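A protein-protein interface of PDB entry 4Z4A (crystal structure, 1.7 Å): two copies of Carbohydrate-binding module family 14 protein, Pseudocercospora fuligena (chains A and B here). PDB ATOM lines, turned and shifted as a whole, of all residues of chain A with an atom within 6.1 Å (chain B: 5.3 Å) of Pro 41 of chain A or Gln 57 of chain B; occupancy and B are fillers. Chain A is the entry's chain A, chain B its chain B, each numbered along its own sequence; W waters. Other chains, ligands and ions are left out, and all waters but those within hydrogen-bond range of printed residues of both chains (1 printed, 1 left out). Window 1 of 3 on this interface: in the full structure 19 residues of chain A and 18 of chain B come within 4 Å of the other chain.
Gln 57 of chain B touches just one residue of chain A: Pro 41 (3.4 Å).
Of the printed residues of chain B, Lys 42 of chain A touches Met 73 (3.9 Å).
Of the printed residues of chain A, His 71 of chain B touches Pro 41.
Of the printed residues of chain A, Ser 59 of chain B touches Leu 39, Gly 40 and Pro 41.
Cys 44 of chain B touches none of the printed residues of chain A.
Tyr 46 of chain B touches none of the printed residues of chain A.
Water W1 bridges the backbone carbonyl oxygen of Pro 41 of chain A and the side-chain amide nitrogen of Gln 57 of chain B.
Ser 59 of chain B touches Gly 40 of chain A.
Pro 41 of chain A touches Gln 57 of chain B (CB to OE1, 3.4 Å).
Pro 41 of chain A touches Ser 59 of chain B (CD to OG, 3.5 Å).
Pro 41 of chain A touches His 71 of chain B.
Met 73 of chain B touches Pro 41 of chain A.
Met 73 of chain B touches Lys 42 of chain A (CE to CE, 3.9 Å).
The side-chain hydroxyl of Ser 59 of chain B is in hydrogen-bond range of the backbone carbonyl oxygen of Leu 39 of chain A.
The backbone carbonyl oxygen of Tyr 55 of chain B is in hydrogen-bond range of the backbone NH of Met 73 of chain B (2.8 Å).
The side-chain sulfur (SG) of Cys 28 of chain B is disulfide-bonded to the side-chain sulfur (SG) of Cys 58 of chain B (2.1 Å).
OG of Ser 59 of chain B lies close to NE2 of His 71 of chain B (3.5 Å).
The backbone NH of Gly 40 of chain A is in hydrogen-bond range of the side-chain carboxylate of Asp 43 of chain A (2.9 Å).
The backbone NH (N) of His 71 of chain B lies within hydrogen-bond range of the backbone carbonyl oxygen (O) of Gln 57 of chain B (2.8 Å).
The backbone carbonyl oxygen (O) of Ser 59 of chain B is in hydrogen-bond range of the backbone NH (N) of Ile 69 of chain B (2.7 Å).
Positions printed for both chains: 45 and 57.
Of the 7 pairs that touch across the chains among the printed residues, none has its exchanged pair printed and touching as well.
Along chain A the printed residues that touch a printed residue of chain B span positions 39 to 42.
Printed residues of chain B that touch a printed residue of chain A: Gln 57, Ser 59, His 71 and Met 73.
Hydrophobic or aromatic side chains of chain B that line the printed part of chain A: His 71 and Met 73.
Among the printed residues, no Asp or Glu carboxylate lies within 4 Å of a Lys or Arg side-chain nitrogen of the other chain.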
ATOM      1  N   CYS A  38     -20.035  -2.185  10.329  1.00  0.00           N
ATOM      2  CA  CYS A  38     -20.493  -3.168   9.356  1.00  0.00           C
ATOM      3  C   CYS A  38     -19.546  -4.345   9.136  1.00  0.00           C
ATOM      4  O   CYS A  38     -19.473  -4.901   8.037  1.00  0.00           O
ATOM      5  CB  CYS A  38     -20.805  -2.457   8.031  1.00  0.00           C
ATOM      6  SG  CYS A  38     -21.998  -1.103   8.223  1.00  0.00           S
ATOM      7  N   LEU A  39     -18.816  -4.749  10.173  1.00  0.00           N
ATOM      8  CA  LEU A  39     -17.780  -5.742   9.996  1.00  0.00           C
ATOM      9  C   LEU A  39     -18.309  -7.161   9.895  1.00  0.00           C
ATOM     10  O   LEU A  39     -17.789  -7.970   9.127  1.00  0.00           O
ATOM     11  CB  LEU A  39     -16.711  -5.674  11.109  1.00  0.00           C
ATOM     12  CG  LEU A  39     -15.875  -4.412  11.170  1.00  0.00           C
ATOM     13  CD1 LEU A  39     -14.947  -4.443  12.384  1.00  0.00           C
ATOM     14  CD2 LEU A  39     -15.068  -4.237   9.901  1.00  0.00           C
ATOM     15  N   GLY A  40     -19.337  -7.469  10.668  1.00  0.00           N
ATOM     16  CA  GLY A  40     -19.765  -8.837  10.810  1.00  0.00           C
ATOM     17  C   GLY A  40     -20.736  -9.234   9.719  1.00  0.00           C
ATOM     18  O   GLY A  40     -21.347  -8.378   9.083  1.00  0.00           O
ATOM     19  N   PRO A  41     -20.908 -10.531   9.503  1.00  0.00           N
ATOM     20  CA  PRO A  41     -21.796 -10.992   8.427  1.00  0.00           C
ATOM     21  C   PRO A  41     -23.236 -10.469   8.432  1.00  0.00           C
ATOM     22  O   PRO A  41     -23.788 -10.223   7.368  1.00  0.00           O
ATOM     23  CB  PRO A  41     -21.789 -12.520   8.598  1.00  0.00           C
ATOM     24  CG  PRO A  41     -20.482 -12.779   9.255  1.00  0.00           C
ATOM     25  CD  PRO A  41     -20.319 -11.663  10.232  1.00  0.00           C
ATOM     26  N   LYS A  42     -23.843 -10.314   9.602  1.00  0.00           N
ATOM     27  CA  LYS A  42     -25.246  -9.907   9.674  1.00  0.00           C
ATOM     28  C   LYS A  42     -25.417  -8.420   9.988  1.00  0.00           C
ATOM     29  O   LYS A  42     -26.533  -7.952  10.226  1.00  0.00           O
ATOM     30  CB  LYS A  42     -25.989 -10.788  10.695  1.00  0.00           C
ATOM     31  CG  LYS A  42     -26.056 -12.263  10.278  1.00  0.00           C
ATOM     32  CD  LYS A  42     -27.117 -12.481   9.199  1.00  0.00           C
ATOM     33  CE  LYS A  42     -26.959 -13.753   8.383  1.00  0.00           C
ATOM     34  NZ  LYS A  42     -27.171 -13.545   6.906  1.00  0.00           N
ATOM     35  N   ASP A  43     -24.322  -7.686  10.021  1.00  0.00           N
ATOM     36  CA  ASP A  43     -24.364  -6.237  10.243  1.00  0.00           C
ATOM     37  C   ASP A  43     -24.781  -5.421   8.999  1.00  0.00           C
ATOM     38  O   ASP A  43     -24.340  -5.693   7.908  1.00  0.00           O
ATOM     39  CB  ASP A  43     -23.007  -5.724  10.736  1.00  0.00           C
ATOM     40  CG  ASP A  43     -22.587  -6.326  12.076  1.00  0.00           C
ATOM     41  OD1 ASP A  43     -23.447  -6.739  12.873  1.00  0.00           O
ATOM     42  OD2 ASP A  43     -21.377  -6.341  12.330  1.00  0.00           O
ATOM     43  N   LEU A  45     -27.624  -4.864   7.318  1.00  0.00           N
ATOM     44  CA  LEU A  45     -28.557  -5.433   6.360  1.00  0.00           C
ATOM     45  C   LEU A  45     -29.990  -5.071   6.778  1.00  0.00           C
ATOM     46  O   LEU A  45     -30.354  -5.134   7.959  1.00  0.00           O
ATOM     47  CB  LEU A  45     -28.417  -6.961   6.334  1.00  0.00           C
ATOM     48  CG  LEU A  45     -27.070  -7.604   6.013  1.00  0.00           C
ATOM     49  CD1 LEU A  45     -27.025  -9.110   6.276  1.00  0.00           C
ATOM     50  CD2 LEU A  45     -26.732  -7.261   4.570  1.00  0.00           C
ATOM     51  N   GLN A  57     -27.885  -3.492   1.700  1.00  0.00           N
ATOM     52  CA  GLN A  57     -26.699  -3.693   2.510  1.00  0.00           C
ATOM     53  C   GLN A  57     -26.027  -2.316   2.514  1.00  0.00           C
ATOM     54  O   GLN A  57     -25.893  -1.733   1.462  1.00  0.00           O
ATOM     55  CB  GLN A  57     -25.775  -4.717   1.911  1.00  0.00           C
ATOM     56  CG  GLN A  57     -24.536  -4.918   2.786  1.00  0.00           C
ATOM     57  CD  GLN A  57     -23.779  -6.159   2.420  1.00  0.00           C
ATOM     58  OE1 GLN A  57     -24.188  -6.908   1.541  1.00  0.00           O
ATOM     59  NE2 GLN A  57     -22.647  -6.353   3.065  1.00  0.00           N
ATOM     60  N   CYS B  28      -8.527 -16.778   6.803  1.00  0.00           N
ATOM     61  CA  CYS B  28      -8.876 -15.731   5.838  1.00  0.00           C
ATOM     62  C   CYS B  28      -7.670 -15.248   5.074  1.00  0.00           C
ATOM     63  O   CYS B  28      -6.649 -15.003   5.668  1.00  0.00           O
ATOM     64  CB  CYS B  28      -9.530 -14.551   6.546  1.00  0.00           C
ATOM     65  SG  CYS B  28     -11.142 -15.077   7.135  1.00  0.00           S
ATOM     66  N   CYS B  44     -14.924 -10.748   0.022  1.00  0.00           N
ATOM     67  CA  CYS B  44     -14.585 -11.562   1.184  1.00  0.00           C
ATOM     68  C   CYS B  44     -15.630 -12.670   1.401  1.00  0.00           C
ATOM     69  O   CYS B  44     -15.875 -13.123   2.522  1.00  0.00           O
ATOM     70  CB  CYS B  44     -14.434 -10.668   2.416  1.00  0.00           C
ATOM     71  SG  CYS B  44     -13.197  -9.370   2.177  1.00  0.00           S
ATOM     72  N   LEU B  45     -16.193 -13.125   0.277  1.00  0.00           N
ATOM     73  CA  LEU B  45     -17.065 -14.295   0.258  1.00  0.00           C
ATOM     74  C   LEU B  45     -16.430 -15.390  -0.571  1.00  0.00           C
ATOM     75  O   LEU B  45     -15.951 -15.140  -1.692  1.00  0.00           O
ATOM     76  CB  LEU B  45     -18.444 -13.931  -0.319  1.00  0.00           C
ATOM     77  CG  LEU B  45     -19.281 -12.898   0.433  1.00  0.00           C
ATOM     78  CD1 LEU B  45     -20.542 -12.532  -0.310  1.00  0.00           C
ATOM     79  CD2 LEU B  45     -19.620 -13.452   1.790  1.00  0.00           C
ATOM     80  N   TYR B  46     -16.521 -16.623  -0.067  1.00  0.00           N
ATOM     81  CA  TYR B  46     -15.798 -17.760  -0.649  1.00  0.00           C
ATOM     82  C   TYR B  46     -16.656 -19.014  -0.544  1.00  0.00           C
ATOM     83  O   TYR B  46     -17.484 -19.116   0.337  1.00  0.00           O
ATOM     84  CB  TYR B  46     -14.499 -18.000   0.142  1.00  0.00           C
ATOM     85  CG  TYR B  46     -13.646 -16.763   0.375  1.00  0.00           C
ATOM     86  CD1 TYR B  46     -13.866 -15.950   1.498  1.00  0.00           C
ATOM     87  CD2 TYR B  46     -12.665 -16.364  -0.522  1.00  0.00           C
ATOM     88  CE1 TYR B  46     -13.113 -14.813   1.723  1.00  0.00           C
ATOM     89  CE2 TYR B  46     -11.937 -15.223  -0.311  1.00  0.00           C
ATOM     90  CZ  TYR B  46     -12.158 -14.453   0.828  1.00  0.00           C
ATOM     91  OH  TYR B  46     -11.446 -13.291   1.042  1.00  0.00           O
ATOM     92  N   TYR B  55     -21.325 -21.304   2.748  1.00  0.00           N
ATOM     93  CA  TYR B  55     -20.184 -20.533   2.239  1.00  0.00           C
ATOM     94  C   TYR B  55     -19.385 -20.002   3.407  1.00  0.00           C
ATOM     95  O   TYR B  55     -19.702 -20.273   4.580  1.00  0.00           O
ATOM     96  CB  TYR B  55     -20.664 -19.371   1.324  1.00  0.00           C
ATOM     97  CG  TYR B  55     -21.587 -18.407   2.044  1.00  0.00           C
ATOM     98  CD1 TYR B  55     -22.942 -18.722   2.258  1.00  0.00           C
ATOM     99  CD2 TYR B  55     -21.122 -17.161   2.477  1.00  0.00           C
ATOM    100  CE1 TYR B  55     -23.774 -17.848   2.919  1.00  0.00           C
ATOM    101  CE2 TYR B  55     -21.950 -16.280   3.140  1.00  0.00           C
ATOM    102  CZ  TYR B  55     -23.283 -16.606   3.336  1.00  0.00           C
ATOM    103  OH  TYR B  55     -24.132 -15.720   3.989  1.00  0.00           O
ATOM    104  N   ILE B  56     -18.290 -19.324   3.087  1.00  0.00           N
ATOM    105  CA  ILE B  56     -17.435 -18.720   4.062  1.00  0.00           C
ATOM    106  C   ILE B  56     -17.432 -17.200   3.823  1.00  0.00           C
ATOM    107  O   ILE B  56     -17.248 -16.739   2.677  1.00  0.00           O
ATOM    108  CB  ILE B  56     -16.014 -19.240   3.950  1.00  0.00           C
ATOM    109  CG1 ILE B  56     -15.966 -20.728   4.366  1.00  0.00           C
ATOM    110  CG2 ILE B  56     -15.058 -18.387   4.807  1.00  0.00           C
ATOM    111  CD1 ILE B  56     -14.611 -21.358   4.134  1.00  0.00           C
ATOM    112  N   GLN B  57     -17.691 -16.451   4.894  1.00  0.00           N
ATOM    113  CA  GLN B  57     -17.474 -14.999   4.871  1.00  0.00           C
ATOM    114  C   GLN B  57     -16.338 -14.686   5.803  1.00  0.00           C
ATOM    115  O   GLN B  57     -16.330 -15.159   6.973  1.00  0.00           O
ATOM    116  CB  GLN B  57     -18.709 -14.249   5.302  1.00  0.00           C
ATOM    117  CG  GLN B  57     -18.555 -12.729   5.284  1.00  0.00           C
ATOM    118  CD  GLN B  57     -19.902 -12.037   5.303  1.00  0.00           C
ATOM    119  OE1 GLN B  57     -20.938 -12.689   5.313  1.00  0.00           O
ATOM    120  NE2 GLN B  57     -19.893 -10.727   5.291  1.00  0.00           N
ATOM    121  N   CYS B  58     -15.380 -13.896   5.310  1.00  0.00           N
ATOM    122  CA  CYS B  58     -14.312 -13.341   6.130  1.00  0.00           C
ATOM    123  C   CYS B  58     -14.666 -11.932   6.561  1.00  0.00           C
ATOM    124  O   CYS B  58     -15.056 -11.102   5.762  1.00  0.00           O
ATOM    125  CB  CYS B  58     -12.979 -13.361   5.395  1.00  0.00           C
ATOM    126  SG  CYS B  58     -12.319 -15.030   5.375  1.00  0.00           S
ATOM    127  N   SER B  59     -14.613 -11.686   7.866  1.00  0.00           N
ATOM    128  CA  SER B  59     -14.855 -10.360   8.399  1.00  0.00           C
ATOM    129  C   SER B  59     -13.531  -9.754   8.824  1.00  0.00           C
ATOM    130  O   SER B  59     -12.730 -10.415   9.462  1.00  0.00           O
ATOM    131  CB  SER B  59     -15.797 -10.410   9.606  1.00  0.00           C
ATOM    132  OG  SER B  59     -17.137 -10.702   9.227  1.00  0.00           O
ATOM    133  N   ILE B  69     -11.450 -12.721  10.192  1.00  0.00           N
ATOM    134  CA  ILE B  69     -12.085 -13.753  10.990  1.00  0.00           C
ATOM    135  C   ILE B  69     -13.028 -14.590  10.129  1.00  0.00           C
ATOM    136  O   ILE B  69     -13.870 -14.033   9.399  1.00  0.00           O
ATOM    137  CB  ILE B  69     -12.873 -13.111  12.142  1.00  0.00           C
ATOM    138  CG1 ILE B  69     -11.928 -12.323  13.058  1.00  0.00           C
ATOM    139  CG2 ILE B  69     -13.636 -14.185  12.911  1.00  0.00           C
ATOM    140  CD1 ILE B  69     -12.662 -11.380  13.985  1.00  0.00           C
ATOM    141  N   ILE B  70     -12.882 -15.922  10.211  1.00  0.00           N
ATOM    142  CA  ILE B  70     -13.688 -16.868   9.427  1.00  0.00           C
ATOM    143  C   ILE B  70     -15.073 -17.002  10.033  1.00  0.00           C
ATOM    144  O   ILE B  70     -15.199 -17.219  11.248  1.00  0.00           O
ATOM    145  CB  ILE B  70     -13.062 -18.305   9.403  1.00  0.00           C
ATOM    146  CG1 ILE B  70     -11.795 -18.340   8.553  1.00  0.00           C
ATOM    147  CG2 ILE B  70     -14.039 -19.377   8.897  1.00  0.00           C
ATOM    148  CD1 ILE B  70     -12.054 -18.476   7.059  1.00  0.00           C
ATOM    149  N   HIS B  71     -16.101 -16.903   9.182  1.00  0.00           N
ATOM    150  CA  HIS B  71     -17.482 -17.280   9.510  1.00  0.00           C
ATOM    151  C   HIS B  71     -17.984 -18.311   8.516  1.00  0.00           C
ATOM    152  O   HIS B  71     -18.034 -18.044   7.313  1.00  0.00           O
ATOM    153  CB  HIS B  71     -18.386 -16.056   9.465  1.00  0.00           C
ATOM    154  CG  HIS B  71     -18.004 -14.998  10.437  1.00  0.00           C
ATOM    155  ND1 HIS B  71     -18.394 -15.039  11.760  1.00  0.00           N
ATOM    156  CD2 HIS B  71     -17.250 -13.883  10.299  1.00  0.00           C
ATOM    157  CE1 HIS B  71     -17.901 -13.991  12.394  1.00  0.00           C
ATOM    158  NE2 HIS B  71     -17.205 -13.273  11.533  1.00  0.00           N
ATOM    159  N   GLU B  72     -18.287 -19.512   8.988  1.00  0.00           N
ATOM    160  CA  GLU B  72     -18.909 -20.546   8.162  1.00  0.00           C
ATOM    161  C   GLU B  72     -20.410 -20.310   8.158  1.00  0.00           C
ATOM    162  O   GLU B  72     -21.087 -20.436   9.166  1.00  0.00           O
ATOM    163  CB  GLU B  72     -18.530 -21.941   8.685  1.00  0.00           C
ATOM    164  CG  GLU B  72     -17.030 -22.165   8.605  1.00  0.00           C
ATOM    165  CD  GLU B  72     -16.620 -23.555   9.066  1.00  0.00           C
ATOM    166  OE1 GLU B  72     -15.881 -23.645  10.062  1.00  0.00           O
ATOM    167  OE2 GLU B  72     -17.038 -24.557   8.442  1.00  0.00           O
ATOM    168  N   MET B  73     -20.939 -19.893   7.018  1.00  0.00           N
ATOM    169  CA  MET B  73     -22.323 -19.463   6.935  1.00  0.00           C
ATOM    170  C   MET B  73     -23.183 -20.492   6.177  1.00  0.00           C
ATOM    171  O   MET B  73     -22.770 -20.983   5.106  1.00  0.00           O
ATOM    172  CB  MET B  73     -22.397 -18.119   6.184  1.00  0.00           C
ATOM    173  CG  MET B  73     -21.526 -16.995   6.739  1.00  0.00           C
ATOM    174  SD  MET B  73     -22.015 -16.450   8.398  1.00  0.00           S
ATOM    175  CE  MET B  73     -23.614 -15.710   8.028  1.00  0.00           C
HETATM  176  O   HOH W   1     -22.442  -9.336   5.241  1.00  0.00           O
